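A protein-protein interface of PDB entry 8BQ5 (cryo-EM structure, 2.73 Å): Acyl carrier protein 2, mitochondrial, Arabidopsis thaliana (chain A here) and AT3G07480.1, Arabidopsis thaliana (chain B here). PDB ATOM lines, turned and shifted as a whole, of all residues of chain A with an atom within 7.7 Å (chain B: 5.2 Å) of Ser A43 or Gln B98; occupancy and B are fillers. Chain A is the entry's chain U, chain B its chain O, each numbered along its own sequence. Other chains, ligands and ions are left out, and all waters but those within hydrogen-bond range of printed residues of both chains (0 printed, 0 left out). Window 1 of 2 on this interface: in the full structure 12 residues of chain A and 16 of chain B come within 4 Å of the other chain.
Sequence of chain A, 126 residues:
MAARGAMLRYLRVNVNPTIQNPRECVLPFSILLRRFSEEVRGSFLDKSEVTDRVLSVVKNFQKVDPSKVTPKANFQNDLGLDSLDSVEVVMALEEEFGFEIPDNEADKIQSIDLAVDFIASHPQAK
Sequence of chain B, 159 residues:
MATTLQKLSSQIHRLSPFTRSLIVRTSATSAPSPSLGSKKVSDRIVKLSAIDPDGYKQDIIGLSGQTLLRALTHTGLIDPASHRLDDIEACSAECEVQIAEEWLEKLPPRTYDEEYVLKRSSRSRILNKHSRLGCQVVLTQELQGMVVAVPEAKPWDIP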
ATOM      1  N   VAL A  40     -24.256  40.316  35.585  1.00  0.00           N
ATOM      2  CA  VAL A  40     -24.695  39.646  34.370  1.00  0.00           C
ATOM      3  C   VAL A  40     -25.226  38.257  34.721  1.00  0.00           C
ATOM      4  O   VAL A  40     -24.785  37.638  35.689  1.00  0.00           O
ATOM      5  CB  VAL A  40     -23.553  39.570  33.331  1.00  0.00           C
ATOM      6  CG1 VAL A  40     -22.470  38.600  33.784  1.00  0.00           C
ATOM      7  CG2 VAL A  40     -24.090  39.193  31.961  1.00  0.00           C
ATOM      8  N   ARG A  41     -26.178  37.771  33.935  1.00  0.00           N
ATOM      9  CA  ARG A  41     -26.814  36.487  34.180  1.00  0.00           C
ATOM     10  C   ARG A  41     -26.336  35.469  33.154  1.00  0.00           C
ATOM     11  O   ARG A  41     -26.298  35.753  31.953  1.00  0.00           O
ATOM     12  CB  ARG A  41     -28.339  36.625  34.139  1.00  0.00           C
ATOM     13  CG  ARG A  41     -29.093  35.348  33.838  1.00  0.00           C
ATOM     14  CD  ARG A  41     -30.593  35.587  33.894  1.00  0.00           C
ATOM     15  NE  ARG A  41     -30.965  36.900  33.378  1.00  0.00           N
ATOM     16  CZ  ARG A  41     -31.190  37.168  32.098  1.00  0.00           C
ATOM     17  NH1 ARG A  41     -31.099  36.233  31.169  1.00  0.00           N
ATOM     18  NH2 ARG A  41     -31.521  38.406  31.744  1.00  0.00           N
ATOM     19  N   GLY A  42     -25.951  34.288  33.634  1.00  0.00           N
ATOM     20  CA  GLY A  42     -25.491  33.216  32.786  1.00  0.00           C
ATOM     21  C   GLY A  42     -26.552  32.140  32.612  1.00  0.00           C
ATOM     22  O   GLY A  42     -27.397  31.905  33.474  1.00  0.00           O
ATOM     23  N   SER A  43     -26.497  31.486  31.455  1.00  0.00           N
ATOM     24  CA  SER A  43     -27.409  30.399  31.151  1.00  0.00           C
ATOM     25  C   SER A  43     -26.712  29.065  30.938  1.00  0.00           C
ATOM     26  O   SER A  43     -27.347  28.132  30.437  1.00  0.00           O
ATOM     27  CB  SER A  43     -28.248  30.731  29.905  1.00  0.00           C
ATOM     28  OG  SER A  43     -29.101  31.836  30.138  1.00  0.00           O
ATOM     29  N   PHE A  44     -25.419  28.974  31.285  1.00  0.00           N
ATOM     30  CA  PHE A  44     -24.681  27.684  31.179  1.00  0.00           C
ATOM     31  C   PHE A  44     -23.643  27.530  32.296  1.00  0.00           C
ATOM     32  O   PHE A  44     -23.116  28.544  32.767  1.00  0.00           O
ATOM     33  CB  PHE A  44     -23.968  27.542  29.832  1.00  0.00           C
ATOM     34  CG  PHE A  44     -24.886  27.429  28.644  1.00  0.00           C
ATOM     35  CD1 PHE A  44     -25.213  28.544  27.893  1.00  0.00           C
ATOM     36  CD2 PHE A  44     -25.445  26.212  28.294  1.00  0.00           C
ATOM     37  CE1 PHE A  44     -26.073  28.444  26.813  1.00  0.00           C
ATOM     38  CE2 PHE A  44     -26.300  26.115  27.208  1.00  0.00           C
ATOM     39  CZ  PHE A  44     -26.613  27.228  26.470  1.00  0.00           C
ATOM     40  N   LEU A  45     -23.383  26.288  32.718  1.00  0.00           N
ATOM     41  CA  LEU A  45     -22.310  26.010  33.707  1.00  0.00           C
ATOM     42  C   LEU A  45     -20.967  26.063  32.967  1.00  0.00           C
ATOM     43  O   LEU A  45     -20.903  25.538  31.838  1.00  0.00           O
ATOM     44  CB  LEU A  45     -22.552  24.625  34.308  1.00  0.00           C
ATOM     45  CG  LEU A  45     -22.987  24.590  35.770  1.00  0.00           C
ATOM     46  CD1 LEU A  45     -24.148  25.538  36.023  1.00  0.00           C
ATOM     47  CD2 LEU A  45     -23.353  23.178  36.189  1.00  0.00           C
ATOM     48  N   ASP A  46     -19.931  26.635  33.588  1.00  0.00           N
ATOM     49  CA  ASP A  46     -18.581  26.722  32.960  1.00  0.00           C
ATOM     50  C   ASP A  46     -18.046  25.320  32.642  1.00  0.00           C
ATOM     51  O   ASP A  46     -18.174  24.437  33.499  1.00  0.00           O
ATOM     52  CB  ASP A  46     -17.617  27.558  33.807  1.00  0.00           C
ATOM     53  CG  ASP A  46     -18.108  28.975  34.031  1.00  0.00           C
ATOM     54  OD1 ASP A  46     -18.743  29.522  33.109  1.00  0.00           O
ATOM     55  OD2 ASP A  46     -17.869  29.513  35.130  1.00  0.00           O
ATOM     56  N   ILE A 119     -23.470  18.112  29.310  1.00  0.00           N
ATOM     57  CA  ILE A 119     -23.905  18.949  30.423  1.00  0.00           C
ATOM     58  C   ILE A 119     -23.453  20.394  30.247  1.00  0.00           C
ATOM     59  O   ILE A 119     -24.182  21.326  30.609  1.00  0.00           O
ATOM     60  CB  ILE A 119     -23.424  18.346  31.756  1.00  0.00           C
ATOM     61  CG1 ILE A 119     -23.858  16.883  31.841  1.00  0.00           C
ATOM     62  CG2 ILE A 119     -23.967  19.127  32.938  1.00  0.00           C
ATOM     63  CD1 ILE A 119     -23.457  16.189  33.114  1.00  0.00           C
ATOM     64  N   ALA A 120     -22.261  20.612  29.689  1.00  0.00           N
ATOM     65  CA  ALA A 120     -21.759  21.969  29.497  1.00  0.00           C
ATOM     66  C   ALA A 120     -22.530  22.745  28.437  1.00  0.00           C
ATOM     67  O   ALA A 120     -22.395  23.971  28.371  1.00  0.00           O
ATOM     68  CB  ALA A 120     -20.276  21.936  29.131  1.00  0.00           C
ATOM     69  N   SER A 121     -23.320  22.069  27.609  1.00  0.00           N
ATOM     70  CA  SER A 121     -24.131  22.727  26.598  1.00  0.00           C
ATOM     71  C   SER A 121     -25.624  22.644  26.880  1.00  0.00           C
ATOM     72  O   SER A 121     -26.415  23.183  26.098  1.00  0.00           O
ATOM     73  CB  SER A 121     -23.837  22.130  25.218  1.00  0.00           C
ATOM     74  OG  SER A 121     -24.200  20.762  25.185  1.00  0.00           O
ATOM     75  N   HIS A 122     -26.033  21.984  27.958  1.00  0.00           N
ATOM     76  CA  HIS A 122     -27.449  21.893  28.295  1.00  0.00           C
ATOM     77  C   HIS A 122     -27.849  23.049  29.205  1.00  0.00           C
ATOM     78  O   HIS A 122     -27.262  23.206  30.281  1.00  0.00           O
ATOM     79  CB  HIS A 122     -27.760  20.566  28.972  1.00  0.00           C
ATOM     80  CG  HIS A 122     -29.145  20.067  28.704  1.00  0.00           C
ATOM     81  ND1 HIS A 122     -30.236  20.471  29.442  1.00  0.00           N
ATOM     82  CD2 HIS A 122     -29.619  19.211  27.769  1.00  0.00           C
ATOM     83  CE1 HIS A 122     -31.321  19.879  28.980  1.00  0.00           C
ATOM     84  NE2 HIS A 122     -30.975  19.108  27.965  1.00  0.00           N
ATOM     85  N   PRO A 123     -28.821  23.877  28.815  1.00  0.00           N
ATOM     86  CA  PRO A 123     -29.230  24.991  29.687  1.00  0.00           C
ATOM     87  C   PRO A 123     -29.848  24.557  31.007  1.00  0.00           C
ATOM     88  O   PRO A 123     -29.706  25.271  32.007  1.00  0.00           O
ATOM     89  CB  PRO A 123     -30.234  25.757  28.816  1.00  0.00           C
ATOM     90  CG  PRO A 123     -30.773  24.732  27.884  1.00  0.00           C
ATOM     91  CD  PRO A 123     -29.621  23.819  27.580  1.00  0.00           C
ATOM     92  N   GLN A 124     -30.531  23.411  31.050  1.00  0.00           N
ATOM     93  CA  GLN A 124     -31.191  22.985  32.280  1.00  0.00           C
ATOM     94  C   GLN A 124     -30.207  22.579  33.370  1.00  0.00           C
ATOM     95  O   GLN A 124     -30.627  22.372  34.514  1.00  0.00           O
ATOM     96  CB  GLN A 124     -32.155  21.831  31.985  1.00  0.00           C
ATOM     97  CG  GLN A 124     -33.433  22.256  31.266  1.00  0.00           C
ATOM     98  CD  GLN A 124     -34.348  21.086  30.953  1.00  0.00           C
ATOM     99  OE1 GLN A 124     -33.898  19.949  30.825  1.00  0.00           O
ATOM    100  NE2 GLN A 124     -35.640  21.362  30.824  1.00  0.00           N
ATOM    101  N   ALA A 125     -28.922  22.452  33.048  1.00  0.00           N
ATOM    102  CA  ALA A 125     -27.918  22.154  34.060  1.00  0.00           C
ATOM    103  C   ALA A 125     -27.749  23.327  35.015  1.00  0.00           C
ATOM    104  O   ALA A 125     -27.697  24.487  34.599  1.00  0.00           O
ATOM    105  CB  ALA A 125     -26.581  21.821  33.399  1.00  0.00           C
ATOM    106  N   GLU B  96     -33.820  35.376  19.866  1.00  0.00           N
ATOM    107  CA  GLU B  96     -32.818  35.164  20.900  1.00  0.00           C
ATOM    108  C   GLU B  96     -32.514  33.686  21.094  1.00  0.00           C
ATOM    109  O   GLU B  96     -33.416  32.848  21.147  1.00  0.00           O
ATOM    110  CB  GLU B  96     -33.288  35.762  22.222  1.00  0.00           C
ATOM    111  CG  GLU B  96     -32.159  36.239  23.099  1.00  0.00           C
ATOM    112  CD  GLU B  96     -32.496  36.172  24.571  1.00  0.00           C
ATOM    113  OE1 GLU B  96     -33.205  37.075  25.061  1.00  0.00           O
ATOM    114  OE2 GLU B  96     -32.046  35.221  25.239  1.00  0.00           O
ATOM    115  N   VAL B  97     -31.223  33.373  21.200  1.00  0.00           N
ATOM    116  CA  VAL B  97     -30.754  32.033  21.522  1.00  0.00           C
ATOM    117  C   VAL B  97     -29.701  32.150  22.614  1.00  0.00           C
ATOM    118  O   VAL B  97     -29.141  33.220  22.856  1.00  0.00           O
ATOM    119  CB  VAL B  97     -30.171  31.296  20.298  1.00  0.00           C
ATOM    120  CG1 VAL B  97     -31.241  31.080  19.249  1.00  0.00           C
ATOM    121  CG2 VAL B  97     -29.001  32.073  19.718  1.00  0.00           C
ATOM    122  N   GLN B  98     -29.447  31.034  23.285  1.00  0.00           N
ATOM    123  CA  GLN B  98     -28.383  30.931  24.272  1.00  0.00           C
ATOM    124  C   GLN B  98     -27.338  29.948  23.771  1.00  0.00           C
ATOM    125  O   GLN B  98     -27.677  28.838  23.351  1.00  0.00           O
ATOM    126  CB  GLN B  98     -28.924  30.487  25.631  1.00  0.00           C
ATOM    127  CG  GLN B  98     -29.529  31.606  26.455  1.00  0.00           C
ATOM    128  CD  GLN B  98     -30.986  31.844  26.136  1.00  0.00           C
ATOM    129  OE1 GLN B  98     -31.760  30.902  25.976  1.00  0.00           O
ATOM    130  NE2 GLN B  98     -31.372  33.111  26.048  1.00  0.00           N
ATOM    131  N   ILE B  99     -26.074  30.355  23.810  1.00  0.00           N
ATOM    132  CA  ILE B  99     -24.987  29.558  23.260  1.00  0.00           C
ATOM    133  C   ILE B  99     -23.902  29.418  24.315  1.00  0.00           C
ATOM    134  O   ILE B  99     -23.525  30.403  24.960  1.00  0.00           O
ATOM    135  CB  ILE B  99     -24.426  30.179  21.969  1.00  0.00           C
ATOM    136  CG1 ILE B  99     -25.554  30.382  20.960  1.00  0.00           C
ATOM    137  CG2 ILE B  99     -23.371  29.280  21.375  1.00  0.00           C
ATOM    138  CD1 ILE B  99     -25.122  30.999  19.660  1.00  0.00           C
ATOM    139  N   ALA B 100     -23.412  28.196  24.496  1.00  0.00           N
ATOM    140  CA  ALA B 100     -22.348  27.963  25.453  1.00  0.00           C
ATOM    141  C   ALA B 100     -21.071  28.662  25.001  1.00  0.00           C
ATOM    142  O   ALA B 100     -20.909  29.034  23.836  1.00  0.00           O
ATOM    143  CB  ALA B 100     -22.102  26.467  25.643  1.00  0.00           C
ATOM    144  N   ASN B 128     -28.036  38.756  29.360  1.00  0.00           N
ATOM    145  CA  ASN B 128     -27.531  37.404  29.551  1.00  0.00           C
ATOM    146  C   ASN B 128     -26.234  37.241  28.767  1.00  0.00           C
ATOM    147  O   ASN B 128     -26.193  37.497  27.561  1.00  0.00           O
ATOM    148  CB  ASN B 128     -28.570  36.378  29.099  1.00  0.00           C
ATOM    149  CG  ASN B 128     -28.237  34.960  29.539  1.00  0.00           C
ATOM    150  OD1 ASN B 128     -27.095  34.515  29.448  1.00  0.00           O
ATOM    151  ND2 ASN B 128     -29.246  34.243  30.018  1.00  0.00           N
ATOM    152  N   HIS B 130     -24.612  34.686  27.778  1.00  0.00           N
ATOM    153  CA  HIS B 130     -24.630  33.651  26.753  1.00  0.00           C
ATOM    154  C   HIS B 130     -25.686  33.898  25.683  1.00  0.00           C
ATOM    155  O   HIS B 130     -25.884  33.043  24.816  1.00  0.00           O
ATOM    156  CB  HIS B 130     -24.850  32.279  27.388  1.00  0.00           C
ATOM    157  CG  HIS B 130     -23.740  31.843  28.291  1.00  0.00           C
ATOM    158  ND1 HIS B 130     -23.898  31.705  29.653  1.00  0.00           N
ATOM    159  CD2 HIS B 130     -22.454  31.513  28.028  1.00  0.00           C
ATOM    160  CE1 HIS B 130     -22.760  31.306  30.189  1.00  0.00           C
ATOM    161  NE2 HIS B 130     -21.865  31.185  29.224  1.00  0.00           N
ATOM    162  N   SER B 131     -26.365  35.039  25.721  1.00  0.00           N
ATOM    163  CA  SER B 131     -27.468  35.304  24.809  1.00  0.00           C
ATOM    164  C   SER B 131     -26.974  35.961  23.528  1.00  0.00           C
ATOM    165  O   SER B 131     -26.113  36.845  23.557  1.00  0.00           O
ATOM    166  CB  SER B 131     -28.517  36.191  25.478  1.00  0.00           C
ATOM    167  OG  SER B 131     -29.486  35.400  26.143  1.00  0.00           O
ATOM    168  N   ARG B 132     -27.529  35.519  22.405  1.00  0.00           N
ATOM    169  CA  ARG B 132     -27.223  36.078  21.100  1.00  0.00           C
ATOM    170  C   ARG B 132     -28.518  36.319  20.343  1.00  0.00           C
ATOM    171  O   ARG B 132     -29.516  35.625  20.553  1.00  0.00           O
ATOM    172  CB  ARG B 132     -26.319  35.146  20.284  1.00  0.00           C
ATOM    173  CG  ARG B 132     -25.018  34.789  20.968  1.00  0.00           C
ATOM    174  CD  ARG B 132     -24.119  36.004  21.076  1.00  0.00           C
ATOM    175  NE  ARG B 132     -24.046  36.731  19.815  1.00  0.00           N
ATOM    176  CZ  ARG B 132     -22.932  36.919  19.123  1.00  0.00           C
ATOM    177  NH1 ARG B 132     -21.768  36.459  19.548  1.00  0.00           N
ATOM    178  NH2 ARG B 132     -22.988  37.587  17.974  1.00  0.00           N
ATOM    179  N   VAL B 147     -23.991  23.663  19.417  1.00  0.00           N
ATOM    180  CA  VAL B 147     -25.229  23.461  20.160  1.00  0.00           C
ATOM    181  C   VAL B 147     -25.799  24.822  20.530  1.00  0.00           C
ATOM    182  O   VAL B 147     -25.073  25.702  21.008  1.00  0.00           O
ATOM    183  CB  VAL B 147     -24.999  22.606  21.416  1.00  0.00           C
ATOM    184  CG1 VAL B 147     -26.333  22.196  22.020  1.00  0.00           C
ATOM    185  CG2 VAL B 147     -24.165  21.385  21.080  1.00  0.00           C
ATOM    186  N   VAL B 148     -27.097  24.994  20.306  1.00  0.00           N
ATOM    187  CA  VAL B 148     -27.799  26.238  20.589  1.00  0.00           C
ATOM    188  C   VAL B 148     -29.003  25.918  21.462  1.00  0.00           C
ATOM    189  O   VAL B 148     -29.669  24.898  21.261  1.00  0.00           O
ATOM    190  CB  VAL B 148     -28.224  26.943  19.283  1.00  0.00           C
ATOM    191  CG1 VAL B 148     -29.443  27.821  19.501  1.00  0.00           C
ATOM    192  CG2 VAL B 148     -27.071  27.759  18.737  1.00  0.00           C
ATOM    193  N   ALA B 149     -29.265  26.769  22.449  1.00  0.00           N
ATOM    194  CA  ALA B 149     -30.418  26.613  23.325  1.00  0.00           C
ATOM    195  C   ALA B 149     -31.503  27.607  22.931  1.00  0.00           C
ATOM    196  O   ALA B 149     -31.254  28.814  22.870  1.00  0.00           O
ATOM    197  CB  ALA B 149     -30.021  26.811  24.787  1.00  0.00           C
ATOM    198  N   VAL B 150     -32.706  27.100  22.677  1.00  0.00           N
ATOM    199  CA  VAL B 150     -33.830  27.920  22.236  1.00  0.00           C
ATOM    200  C   VAL B 150     -34.683  28.242  23.461  1.00  0.00           C
ATOM    201  O   VAL B 150     -35.317  27.331  24.016  1.00  0.00           O
ATOM    202  CB  VAL B 150     -34.655  27.209  21.157  1.00  0.00           C
ATOM    203  CG1 VAL B 150     -35.916  28.002  20.839  1.00  0.00           C
ATOM    204  CG2 VAL B 150     -33.817  26.999  19.911  1.00  0.00           C
ATOM    205  N   PRO B 151     -34.741  29.493  23.904  1.00  0.00           N
ATOM    206  CA  PRO B 151     -35.561  29.836  25.067  1.00  0.00           C
ATOM    207  C   PRO B 151     -37.040  29.888  24.706  1.00  0.00           C
ATOM    208  O   PRO B 151     -37.431  29.821  23.541  1.00  0.00           O
ATOM    209  CB  PRO B 151     -35.040  31.218  25.469  1.00  0.00           C
ATOM    210  CG  PRO B 151     -34.561  31.808  24.198  1.00  0.00           C
ATOM    211  CD  PRO B 151     -34.041  30.667  23.356  1.00  0.00           C
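The side-chain amide oxygen (OD1) of Asn B128 sits close to the backbone carbonyl oxygen (O) of Arg A41, at 2.9 Å. The side-chain amide nitrogen (ND2) of Asn B128 sits at hydrogen-bond distance from the side-chain hydroxyl (OG) of Ser A43, 2.4 Å away. The backbone NH (N) of Ser A43 is in hydrogen-bond range of a ring nitrogen (ND1) of His B130 (3.2 Å).
Of the printed residues of chain B, Gly A42 touches Asn B128 (3.9 Å) and His B130 (3.8 Å). Of chain B, only Gln B98 (3.7 Å), Asn B128 (2.4 Å) and His B130 (3.2 Å) come within 4 Å of Ser A43. Gln B98 touches two residues of chain A. Of the printed residues of chain A, Ala B149 touches Phe A44 and Pro A123. The nearest printed residue of chain A that does not touch Ala B100 is Ser A121 (4.4 Å).
Hydrophobic or aromatic side chains of chain A within 4 Å of the printed part of chain B: Phe A44 and Pro A123. Of the 14 printed residues of chain B, 6 touch a printed residue of chain A. Hydrophobic or aromatic side chains of chain B that line the printed part of chain A: Ala B100, His B130 and Ala B149. Among the printed residues, 13 pairs touch across the chains. Among the printed residues, no Asp or Glu carboxylate lies within 4 Å of a Lys or Arg side-chain nitrogen of the other chain.
The side-chain hydroxyl of Ser B131 lies within hydrogen-bond range of the side-chain amide nitrogen of Gln B98, 3.0 Å away. The backbone carbonyl oxygen (O) of Gln B98 is in hydrogen-bond range of the backbone NH (N) of Ala B149 (2.8 Å). O of His B130 is in hydrogen-bond range of N of Ile B99. The backbone NH (N) of His B130 sits at hydrogen-bond distance from the side-chain amide oxygen (OD1) of Asn B128 (3.0 Å).
Asn B128 touches Gly A42 (OD1 to CA, 3.9 Å). Gly A42 touches His B130. OG of Ser A43 touches CG of Gln B98, 3.7 Å away. CE1 of Phe A44 touches C of Gln B98 (3.6 Å). Ile B99 touches Phe A44 (C to CE1, 3.4 Å). CE1 of Phe A44 touches N of Ala B100, 3.5 Å away. His B130 touches Phe A44 (ND1 to N, 3.5 Å). Phe A44 touches Ala B149 (CZ to CB, 3.8 Å). Ala A120 touches Ala B100 (O to CB, 3.7 Å). CB of Ala B149 touches CG of Pro A123 (3.8 Å).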
